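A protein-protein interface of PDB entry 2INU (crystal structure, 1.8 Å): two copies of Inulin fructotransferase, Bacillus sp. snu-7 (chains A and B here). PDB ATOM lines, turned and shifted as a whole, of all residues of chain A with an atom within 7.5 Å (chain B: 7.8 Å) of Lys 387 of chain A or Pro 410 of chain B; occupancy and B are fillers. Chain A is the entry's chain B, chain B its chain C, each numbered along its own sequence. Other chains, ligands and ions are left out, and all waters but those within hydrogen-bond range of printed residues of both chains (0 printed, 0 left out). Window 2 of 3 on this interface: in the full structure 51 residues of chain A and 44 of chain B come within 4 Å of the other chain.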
ATOM      1  N   ASN A 327     -16.248   5.530   6.130  1.00  0.00           N
ATOM      2  CA  ASN A 327     -14.906   5.345   5.588  1.00  0.00           C
ATOM      3  C   ASN A 327     -13.914   6.143   6.432  1.00  0.00           C
ATOM      4  O   ASN A 327     -14.274   7.188   6.988  1.00  0.00           O
ATOM      5  CB  ASN A 327     -14.862   5.804   4.126  1.00  0.00           C
ATOM      6  CG  ASN A 327     -15.820   5.026   3.241  1.00  0.00           C
ATOM      7  OD1 ASN A 327     -15.617   3.840   2.974  1.00  0.00           O
ATOM      8  ND2 ASN A 327     -16.871   5.693   2.780  1.00  0.00           N
ATOM      9  N   LEU A 328     -12.679   5.652   6.537  1.00  0.00           N
ATOM     10  CA  LEU A 328     -11.655   6.332   7.326  1.00  0.00           C
ATOM     11  C   LEU A 328     -10.464   6.753   6.464  1.00  0.00           C
ATOM     12  O   LEU A 328      -9.653   5.910   6.050  1.00  0.00           O
ATOM     13  CB  LEU A 328     -11.149   5.430   8.462  1.00  0.00           C
ATOM     14  CG  LEU A 328      -9.892   5.929   9.197  1.00  0.00           C
ATOM     15  CD1 LEU A 328     -10.229   7.157  10.026  1.00  0.00           C
ATOM     16  CD2 LEU A 328      -9.351   4.824  10.087  1.00  0.00           C
ATOM     17  N   ILE A 329     -10.356   8.056   6.220  1.00  0.00           N
ATOM     18  CA  ILE A 329      -9.266   8.607   5.433  1.00  0.00           C
ATOM     19  C   ILE A 329      -8.326   9.280   6.426  1.00  0.00           C
ATOM     20  O   ILE A 329      -8.632  10.363   6.940  1.00  0.00           O
ATOM     21  CB  ILE A 329      -9.790   9.645   4.415  1.00  0.00           C
ATOM     22  CG1 ILE A 329     -10.888   9.020   3.558  1.00  0.00           C
ATOM     23  CG2 ILE A 329      -8.656  10.132   3.533  1.00  0.00           C
ATOM     24  CD1 ILE A 329     -12.281   9.114   4.160  1.00  0.00           C
ATOM     25  N   ILE A 355     -15.993  15.054   0.823  1.00  0.00           N
ATOM     26  CA  ILE A 355     -16.895  14.048   1.342  1.00  0.00           C
ATOM     27  C   ILE A 355     -18.232  14.429   0.696  1.00  0.00           C
ATOM     28  O   ILE A 355     -19.023  15.192   1.247  1.00  0.00           O
ATOM     29  CB  ILE A 355     -16.902  14.124   2.887  1.00  0.00           C
ATOM     30  CG1 ILE A 355     -15.472  13.907   3.404  1.00  0.00           C
ATOM     31  CG2 ILE A 355     -17.819  13.077   3.479  1.00  0.00           C
ATOM     32  CD1 ILE A 355     -14.861  12.550   3.021  1.00  0.00           C
ATOM     33  N   ALA A 360     -21.189   9.320   8.735  1.00  0.00           N
ATOM     34  CA  ALA A 360     -20.111   8.893   9.618  1.00  0.00           C
ATOM     35  C   ALA A 360     -18.685   8.830   9.086  1.00  0.00           C
ATOM     36  O   ALA A 360     -17.831   8.198   9.716  1.00  0.00           O
ATOM     37  CB  ALA A 360     -20.469   7.553  10.203  1.00  0.00           C
ATOM     38  N   ASN A 361     -18.390   9.476   7.966  1.00  0.00           N
ATOM     39  CA  ASN A 361     -17.028   9.406   7.492  1.00  0.00           C
ATOM     40  C   ASN A 361     -16.110  10.132   8.457  1.00  0.00           C
ATOM     41  O   ASN A 361     -16.494  11.129   9.076  1.00  0.00           O
ATOM     42  CB  ASN A 361     -16.939   9.943   6.072  1.00  0.00           C
ATOM     43  CG  ASN A 361     -17.696   9.067   5.096  1.00  0.00           C
ATOM     44  OD1 ASN A 361     -17.259   7.963   4.765  1.00  0.00           O
ATOM     45  ND2 ASN A 361     -18.846   9.550   4.638  1.00  0.00           N
ATOM     46  N   VAL A 362     -14.907   9.589   8.615  1.00  0.00           N
ATOM     47  CA  VAL A 362     -13.926  10.151   9.530  1.00  0.00           C
ATOM     48  C   VAL A 362     -12.653  10.545   8.797  1.00  0.00           C
ATOM     49  O   VAL A 362     -12.078   9.744   8.051  1.00  0.00           O
ATOM     50  CB  VAL A 362     -13.593   9.129  10.634  1.00  0.00           C
ATOM     51  CG1 VAL A 362     -12.561   9.694  11.589  1.00  0.00           C
ATOM     52  CG2 VAL A 362     -14.870   8.751  11.378  1.00  0.00           C
ATOM     53  N   VAL A 363     -12.225  11.786   9.009  1.00  0.00           N
ATOM     54  CA  VAL A 363     -11.028  12.305   8.375  1.00  0.00           C
ATOM     55  C   VAL A 363     -10.062  12.801   9.447  1.00  0.00           C
ATOM     56  O   VAL A 363     -10.303  13.832  10.083  1.00  0.00           O
ATOM     57  CB  VAL A 363     -11.400  13.442   7.406  1.00  0.00           C
ATOM     58  CG1 VAL A 363     -10.157  14.048   6.807  1.00  0.00           C
ATOM     59  CG2 VAL A 363     -12.323  12.904   6.323  1.00  0.00           C
ATOM     60  N   ALA A 364      -8.971  12.062   9.643  1.00  0.00           N
ATOM     61  CA  ALA A 364      -7.984  12.418  10.657  1.00  0.00           C
ATOM     62  C   ALA A 364      -6.532  12.378  10.179  1.00  0.00           C
ATOM     63  O   ALA A 364      -6.161  11.576   9.317  1.00  0.00           O
ATOM     64  CB  ALA A 364      -8.147  11.513  11.866  1.00  0.00           C
ATOM     65  N   VAL A 377     -10.463  19.967   3.571  1.00  0.00           N
ATOM     66  CA  VAL A 377     -11.595  19.078   3.663  1.00  0.00           C
ATOM     67  C   VAL A 377     -12.885  19.833   3.447  1.00  0.00           C
ATOM     68  O   VAL A 377     -13.084  20.925   3.978  1.00  0.00           O
ATOM     69  CB  VAL A 377     -11.641  18.370   5.038  1.00  0.00           C
ATOM     70  CG1 VAL A 377     -12.698  17.282   5.023  1.00  0.00           C
ATOM     71  CG2 VAL A 377     -10.276  17.794   5.373  1.00  0.00           C
ATOM     72  N   LEU A 379     -17.054  19.075   3.423  1.00  0.00           N
ATOM     73  CA  LEU A 379     -18.135  18.151   3.702  1.00  0.00           C
ATOM     74  C   LEU A 379     -19.363  18.777   3.079  1.00  0.00           C
ATOM     75  O   LEU A 379     -19.834  19.835   3.509  1.00  0.00           O
ATOM     76  CB  LEU A 379     -18.330  17.995   5.205  1.00  0.00           C
ATOM     77  CG  LEU A 379     -17.209  17.451   6.011  1.00  0.00           C
ATOM     78  CD1 LEU A 379     -16.479  16.401   5.356  1.00  0.00           C
ATOM     79  CD2 LEU A 379     -16.073  18.442   6.217  1.00  0.00           C
ATOM     80  N   THR A 384     -23.579  13.652   6.809  1.00  0.00           N
ATOM     81  CA  THR A 384     -24.061  13.670   8.172  1.00  0.00           C
ATOM     82  C   THR A 384     -23.071  12.984   9.092  1.00  0.00           C
ATOM     83  O   THR A 384     -22.388  12.022   8.704  1.00  0.00           O
ATOM     84  CB  THR A 384     -25.404  12.933   8.349  1.00  0.00           C
ATOM     85  OG1 THR A 384     -25.278  11.572   7.906  1.00  0.00           O
ATOM     86  CG2 THR A 384     -26.511  13.633   7.580  1.00  0.00           C
ATOM     87  N   HIS A 385     -22.990  13.523  10.304  1.00  0.00           N
ATOM     88  CA  HIS A 385     -22.146  12.999  11.365  1.00  0.00           C
ATOM     89  C   HIS A 385     -20.676  12.701  11.018  1.00  0.00           C
ATOM     90  O   HIS A 385     -20.089  11.749  11.530  1.00  0.00           O
ATOM     91  CB  HIS A 385     -22.859  11.771  11.940  1.00  0.00           C
ATOM     92  CG  HIS A 385     -24.320  11.982  12.120  1.00  0.00           C
ATOM     93  ND1 HIS A 385     -24.854  12.960  12.925  1.00  0.00           N
ATOM     94  CD2 HIS A 385     -25.404  11.357  11.545  1.00  0.00           C
ATOM     95  CE1 HIS A 385     -26.174  12.945  12.849  1.00  0.00           C
ATOM     96  NE2 HIS A 385     -26.518  11.981  12.019  1.00  0.00           N
ATOM     97  N   SER A 386     -20.082  13.544  10.171  1.00  0.00           N
ATOM     98  CA  SER A 386     -18.678  13.398   9.762  1.00  0.00           C
ATOM     99  C   SER A 386     -17.760  13.855  10.893  1.00  0.00           C
ATOM    100  O   SER A 386     -18.179  14.631  11.758  1.00  0.00           O
ATOM    101  CB  SER A 386     -18.380  14.246   8.521  1.00  0.00           C
ATOM    102  OG  SER A 386     -19.297  13.985   7.472  1.00  0.00           O
ATOM    103  N   LYS A 387     -16.514  13.381  10.884  1.00  0.00           N
ATOM    104  CA  LYS A 387     -15.537  13.753  11.917  1.00  0.00           C
ATOM    105  C   LYS A 387     -14.245  14.220  11.250  1.00  0.00           C
ATOM    106  O   LYS A 387     -13.642  13.473  10.470  1.00  0.00           O
ATOM    107  CB  LYS A 387     -15.184  12.552  12.800  1.00  0.00           C
ATOM    108  CG  LYS A 387     -16.359  11.825  13.417  1.00  0.00           C
ATOM    109  CD  LYS A 387     -16.826  12.467  14.706  1.00  0.00           C
ATOM    110  CE  LYS A 387     -17.854  11.577  15.387  1.00  0.00           C
ATOM    111  NZ  LYS A 387     -18.557  12.295  16.476  1.00  0.00           N
ATOM    112  N   VAL A 388     -13.811  15.438  11.553  1.00  0.00           N
ATOM    113  CA  VAL A 388     -12.573  15.939  10.978  1.00  0.00           C
ATOM    114  C   VAL A 388     -11.616  16.322  12.097  1.00  0.00           C
ATOM    115  O   VAL A 388     -11.870  17.265  12.864  1.00  0.00           O
ATOM    116  CB  VAL A 388     -12.829  17.146  10.054  1.00  0.00           C
ATOM    117  CG1 VAL A 388     -11.522  17.592   9.409  1.00  0.00           C
ATOM    118  CG2 VAL A 388     -13.835  16.769   8.981  1.00  0.00           C
ATOM    119  N   LEU A 389     -10.521  15.567  12.179  1.00  0.00           N
ATOM    120  CA  LEU A 389      -9.510  15.775  13.203  1.00  0.00           C
ATOM    121  C   LEU A 389      -8.136  16.024  12.614  1.00  0.00           C
ATOM    122  O   LEU A 389      -7.675  15.277  11.736  1.00  0.00           O
ATOM    123  CB  LEU A 389      -9.363  14.547  14.098  1.00  0.00           C
ATOM    124  CG  LEU A 389     -10.535  13.666  14.497  1.00  0.00           C
ATOM    125  CD1 LEU A 389     -10.008  12.538  15.378  1.00  0.00           C
ATOM    126  CD2 LEU A 389     -11.559  14.478  15.236  1.00  0.00           C
ATOM    127  N   SER A 391      -6.762  17.840  10.393  1.00  0.00           N
ATOM    128  CA  SER A 391      -6.630  17.808   8.943  1.00  0.00           C
ATOM    129  C   SER A 391      -6.707  19.227   8.389  1.00  0.00           C
ATOM    130  O   SER A 391      -7.062  19.433   7.224  1.00  0.00           O
ATOM    131  CB  SER A 391      -7.724  16.934   8.322  1.00  0.00           C
ATOM    132  OG  SER A 391      -7.472  15.566   8.575  1.00  0.00           O
ATOM    133  N   ASP A 403     -23.885  18.914  11.800  1.00  0.00           N
ATOM    134  CA  ASP A 403     -23.598  17.911  12.815  1.00  0.00           C
ATOM    135  C   ASP A 403     -22.147  17.466  12.687  1.00  0.00           C
ATOM    136  O   ASP A 403     -21.733  16.478  13.310  1.00  0.00           O
ATOM    137  CB  ASP A 403     -24.523  16.699  12.698  1.00  0.00           C
ATOM    138  CG  ASP A 403     -24.967  16.437  11.276  1.00  0.00           C
ATOM    139  OD1 ASP A 403     -24.100  16.204  10.401  1.00  0.00           O
ATOM    140  OD2 ASP A 403     -26.192  16.464  11.024  1.00  0.00           O
ATOM    141  N   THR A 404     -21.372  18.195  11.889  1.00  0.00           N
ATOM    142  CA  THR A 404     -19.980  17.845  11.718  1.00  0.00           C
ATOM    143  C   THR A 404     -19.199  18.211  12.965  1.00  0.00           C
ATOM    144  O   THR A 404     -19.397  19.283  13.552  1.00  0.00           O
ATOM    145  CB  THR A 404     -19.346  18.576  10.532  1.00  0.00           C
ATOM    146  OG1 THR A 404     -19.959  18.140   9.310  1.00  0.00           O
ATOM    147  CG2 THR A 404     -17.851  18.287  10.485  1.00  0.00           C
ATOM    148  N   ALA A 405     -18.320  17.305  13.376  1.00  0.00           N
ATOM    149  CA  ALA A 405     -17.474  17.541  14.537  1.00  0.00           C
ATOM    150  C   ALA A 405     -16.081  17.778  13.968  1.00  0.00           C
ATOM    151  O   ALA A 405     -15.536  16.922  13.260  1.00  0.00           O
ATOM    152  CB  ALA A 405     -17.480  16.332  15.446  1.00  0.00           C
ATOM    153  N   ILE A 406     -15.520  18.944  14.270  1.00  0.00           N
ATOM    154  CA  ILE A 406     -14.211  19.322  13.760  1.00  0.00           C
ATOM    155  C   ILE A 406     -13.228  19.676  14.873  1.00  0.00           C
ATOM    156  O   ILE A 406     -13.584  20.357  15.834  1.00  0.00           O
ATOM    157  CB  ILE A 406     -14.320  20.564  12.845  1.00  0.00           C
ATOM    158  CG1 ILE A 406     -15.143  20.237  11.604  1.00  0.00           C
ATOM    159  CG2 ILE A 406     -12.931  21.063  12.455  1.00  0.00           C
ATOM    160  CD1 ILE A 406     -15.358  21.418  10.678  1.00  0.00           C
ATOM    161  N   ARG A 407     -11.991  19.204  14.744  1.00  0.00           N
ATOM    162  CA  ARG A 407     -10.943  19.526  15.713  1.00  0.00           C
ATOM    163  C   ARG A 407      -9.776  20.126  14.952  1.00  0.00           C
ATOM    164  O   ARG A 407      -9.134  19.448  14.154  1.00  0.00           O
ATOM    165  CB  ARG A 407     -10.461  18.296  16.479  1.00  0.00           C
ATOM    166  CG  ARG A 407      -9.375  18.656  17.504  1.00  0.00           C
ATOM    167  CD  ARG A 407      -9.004  17.482  18.392  1.00  0.00           C
ATOM    168  NE  ARG A 407      -8.242  16.470  17.665  1.00  0.00           N
ATOM    169  CZ  ARG A 407      -8.227  15.185  18.002  1.00  0.00           C
ATOM    170  NH1 ARG A 407      -8.933  14.763  19.047  1.00  0.00           N
ATOM    171  NH2 ARG A 407      -7.502  14.323  17.308  1.00  0.00           N
ATOM    172  N   HIS B 367     -11.268   3.557  14.174  1.00  0.00           N
ATOM    173  CA  HIS B 367     -12.660   3.755  13.814  1.00  0.00           C
ATOM    174  C   HIS B 367     -13.467   2.468  13.924  1.00  0.00           C
ATOM    175  O   HIS B 367     -13.120   1.452  13.312  1.00  0.00           O
ATOM    176  CB  HIS B 367     -12.766   4.312  12.391  1.00  0.00           C
ATOM    177  CG  HIS B 367     -14.156   4.632  11.971  1.00  0.00           C
ATOM    178  ND1 HIS B 367     -14.633   4.403  10.698  1.00  0.00           N
ATOM    179  CD2 HIS B 367     -15.199   5.191  12.657  1.00  0.00           C
ATOM    180  CE1 HIS B 367     -15.886   4.799  10.614  1.00  0.00           C
ATOM    181  NE2 HIS B 367     -16.251   5.279  11.783  1.00  0.00           N
ATOM    182  N   LEU B 389      -6.941   7.489  22.710  1.00  0.00           N
ATOM    183  CA  LEU B 389      -7.197   8.728  21.983  1.00  0.00           C
ATOM    184  C   LEU B 389      -8.003   8.501  20.718  1.00  0.00           C
ATOM    185  O   LEU B 389      -7.688   7.606  19.918  1.00  0.00           O
ATOM    186  CB  LEU B 389      -5.896   9.384  21.532  1.00  0.00           C
ATOM    187  CG  LEU B 389      -4.612   9.340  22.345  1.00  0.00           C
ATOM    188  CD1 LEU B 389      -3.535  10.100  21.582  1.00  0.00           C
ATOM    189  CD2 LEU B 389      -4.838   9.961  23.696  1.00  0.00           C
ATOM    190  N   ASP B 390      -9.027   9.324  20.525  1.00  0.00           N
ATOM    191  CA  ASP B 390      -9.834   9.256  19.316  1.00  0.00           C
ATOM    192  C   ASP B 390     -10.206   7.844  18.874  1.00  0.00           C
ATOM    193  O   ASP B 390     -10.070   7.494  17.702  1.00  0.00           O
ATOM    194  CB  ASP B 390      -9.081   9.990  18.208  1.00  0.00           C
ATOM    195  CG  ASP B 390      -8.570  11.336  18.672  1.00  0.00           C
ATOM    196  OD1 ASP B 390      -9.340  12.054  19.354  1.00  0.00           O
ATOM    197  OD2 ASP B 390      -7.420  11.699  18.347  1.00  0.00           O
ATOM    198  N   SER B 391     -10.692   7.041  19.818  1.00  0.00           N
ATOM    199  CA  SER B 391     -11.097   5.675  19.516  1.00  0.00           C
ATOM    200  C   SER B 391     -12.504   5.432  20.048  1.00  0.00           C
ATOM    201  O   SER B 391     -12.895   4.290  20.308  1.00  0.00           O
ATOM    202  CB  SER B 391     -10.116   4.677  20.136  1.00  0.00           C
ATOM    203  OG  SER B 391      -8.864   4.724  19.475  1.00  0.00           O
ATOM    204  N   GLY B 392     -13.263   6.515  20.204  1.00  0.00           N
ATOM    205  CA  GLY B 392     -14.629   6.393  20.683  1.00  0.00           C
ATOM    206  C   GLY B 392     -15.034   7.473  21.672  1.00  0.00           C
ATOM    207  O   GLY B 392     -14.178   8.130  22.284  1.00  0.00           O
ATOM    208  N   THR B 393     -16.343   7.658  21.838  1.00  0.00           N
ATOM    209  CA  THR B 393     -16.847   8.649  22.779  1.00  0.00           C
ATOM    210  C   THR B 393     -16.623   8.068  24.159  1.00  0.00           C
ATOM    211  O   THR B 393     -16.298   6.893  24.290  1.00  0.00           O
ATOM    212  CB  THR B 393     -18.352   8.919  22.573  1.00  0.00           C
ATOM    213  OG1 THR B 393     -19.068   7.680  22.600  1.00  0.00           O
ATOM    214  CG2 THR B 393     -18.580   9.624  21.242  1.00  0.00           C
ATOM    215  N   GLN B 396     -18.285   4.831  24.863  1.00  0.00           N
ATOM    216  CA  GLN B 396     -17.955   3.714  23.987  1.00  0.00           C
ATOM    217  C   GLN B 396     -16.639   3.135  24.502  1.00  0.00           C
ATOM    218  O   GLN B 396     -16.104   2.173  23.941  1.00  0.00           O
ATOM    219  CB  GLN B 396     -17.811   4.191  22.535  1.00  0.00           C
ATOM    220  CG  GLN B 396     -19.135   4.721  21.920  1.00  0.00           C
ATOM    221  CD  GLN B 396     -18.983   5.261  20.504  1.00  0.00           C
ATOM    222  OE1 GLN B 396     -18.009   5.948  20.184  1.00  0.00           O
ATOM    223  NE2 GLN B 396     -19.967   4.974  19.657  1.00  0.00           N
ATOM    224  N   ARG B 407      -9.163  10.414  25.666  1.00  0.00           N
ATOM    225  CA  ARG B 407      -9.546  11.618  24.930  1.00  0.00           C
ATOM    226  C   ARG B 407     -10.644  11.247  23.953  1.00  0.00           C
ATOM    227  O   ARG B 407     -10.413  10.494  23.010  1.00  0.00           O
ATOM    228  CB  ARG B 407      -8.372  12.223  24.167  1.00  0.00           C
ATOM    229  CG  ARG B 407      -8.790  13.491  23.405  1.00  0.00           C
ATOM    230  CD  ARG B 407      -7.606  14.182  22.755  1.00  0.00           C
ATOM    231  NE  ARG B 407      -7.122  13.453  21.585  1.00  0.00           N
ATOM    232  CZ  ARG B 407      -5.869  13.511  21.150  1.00  0.00           C
ATOM    233  NH1 ARG B 407      -4.979  14.260  21.790  1.00  0.00           N
ATOM    234  NH2 ARG B 407      -5.504  12.828  20.079  1.00  0.00           N
ATOM    235  N   PRO B 408     -11.865  11.738  24.197  1.00  0.00           N
ATOM    236  CA  PRO B 408     -13.013  11.459  23.339  1.00  0.00           C
ATOM    237  C   PRO B 408     -12.837  11.769  21.862  1.00  0.00           C
ATOM    238  O   PRO B 408     -12.110  12.680  21.481  1.00  0.00           O
ATOM    239  CB  PRO B 408     -14.095  12.341  23.924  1.00  0.00           C
ATOM    240  CG  PRO B 408     -13.823  12.304  25.357  1.00  0.00           C
ATOM    241  CD  PRO B 408     -12.297  12.358  25.467  1.00  0.00           C
ATOM    242  N   THR B 409     -13.497  10.983  21.022  1.00  0.00           N
ATOM    243  CA  THR B 409     -13.488  11.278  19.597  1.00  0.00           C
ATOM    244  C   THR B 409     -14.540  12.367  19.791  1.00  0.00           C
ATOM    245  O   THR B 409     -15.607  12.096  20.346  1.00  0.00           O
ATOM    246  CB  THR B 409     -14.091  10.158  18.740  1.00  0.00           C
ATOM    247  OG1 THR B 409     -13.276   8.983  18.831  1.00  0.00           O
ATOM    248  CG2 THR B 409     -14.153  10.601  17.285  1.00  0.00           C
ATOM    249  N   PRO B 410     -14.253  13.609  19.391  1.00  0.00           N
ATOM    250  CA  PRO B 410     -15.255  14.656  19.592  1.00  0.00           C
ATOM    251  C   PRO B 410     -16.690  14.283  19.230  1.00  0.00           C
ATOM    252  O   PRO B 410     -16.907  13.389  18.373  1.00  0.00           O
ATOM    253  CB  PRO B 410     -14.717  15.800  18.759  1.00  0.00           C
ATOM    254  CG  PRO B 410     -13.243  15.692  19.067  1.00  0.00           C
ATOM    255  CD  PRO B 410     -12.961  14.195  18.993  1.00  0.00           C
ATOM    256  OXT PRO B 410     -17.610  14.883  19.832  1.00  0.00           O
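O of Asn 327 of chain A is in hydrogen-bond range of N of Val 362 of chain A (3.0 Å).
The backbone carbonyl oxygen (O) of Val 362 of chain A is in hydrogen-bond range of the backbone NH (N) of Ile 329 of chain A.
The backbone NH (N) of Lys 387 of chain A lies within hydrogen-bond range of the backbone carbonyl oxygen (O) of Asn 361 of chain A (2.9 Å).
N of Val 363 of chain A lies within hydrogen-bond range of O of Lys 387 of chain A.
N of Leu 389 of chain A is in hydrogen-bond range of O of Val 363 of chain A, 2.7 Å away.
The backbone carbonyl oxygen (O) of Val 388 of chain A lies within hydrogen-bond range of the backbone NH (N) of Arg 407 of chain A, at 2.7 Å.
Among the printed residues, pairs that only touch across the chains: Ala 360 of chain A with His 367 of chain B (3.9 Å), Val 362 of chain A with His 367 of chain B (3.8 Å) and Leu 389 of chain A with Asp 390 of chain B (3.8 Å).
Arg 407 of chain A touches its own counterpart, Arg 407 of chain B.
Positions printed for both chains: 389, 391 and 407.
Of the 6 pairs that touch across the chains among the printed residues, 1 has its exchanged pair printed and touching as well.
Lys 387 of chain A touches one residue of chain B.
Of chain A, only Lys 387 (2.7 Å) comes within 4 Å of Pro 410 of chain B.
Of the printed residues of chain B, Val 362 of chain A touches His 367.
Printed residues of chain A within 4 Å of Arg 407 of chain B: Arg 407.
Of the printed residues of chain B, Leu 389 of chain A touches Asp 390 (3.8 Å).
Printed residues of chain A within 4 Å of Asp 390 of chain B: Leu 389 and Arg 407.
Printed residues of chain B within 4 Å of Ala 360 of chain A: His 367.
The nearest residue of chain B that does not touch Lys 387 of chain A is Thr 409 of chain B (4.2 Å).
The nearest residue of chain A that does not touch Pro 410 of chain B is Leu 389 of chain A (4.02 Å).
The nearest printed residue of chain A that does not touch Arg 407 of chain B is Leu 389 of chain A (6.5 Å).
The chain-end carboxylate (O) of Pro 410 of chain B lies within salt-bridge range of the side-chain amino group (NZ) of Lys 387 of chain A (2.7 Å).
The side-chain carboxylate (OD1) of Asp 390 of chain B is in salt-bridge range of the guanidinium group (NH1) of Arg 407 of chain A (2.8 Å).
The guanidinium group (NH1) of Arg 407 of chain A lies close to the guanidinium group (NE) of Arg 407 of chain B (3.4 Å).
Of the 23 printed residues of chain A, 5 touch a printed residue of chain B.
Printed residues of chain A that touch a printed residue of chain B: Ala 360, Val 362, Lys 387, Leu 389 and Arg 407.
Hydrophobic or aromatic side chains of chain A within 4 Å of the printed part of chain B: Val 362 and Leu 389.
Hydrophobic or aromatic side chains of chain B that line the printed part of chain A: His 367.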
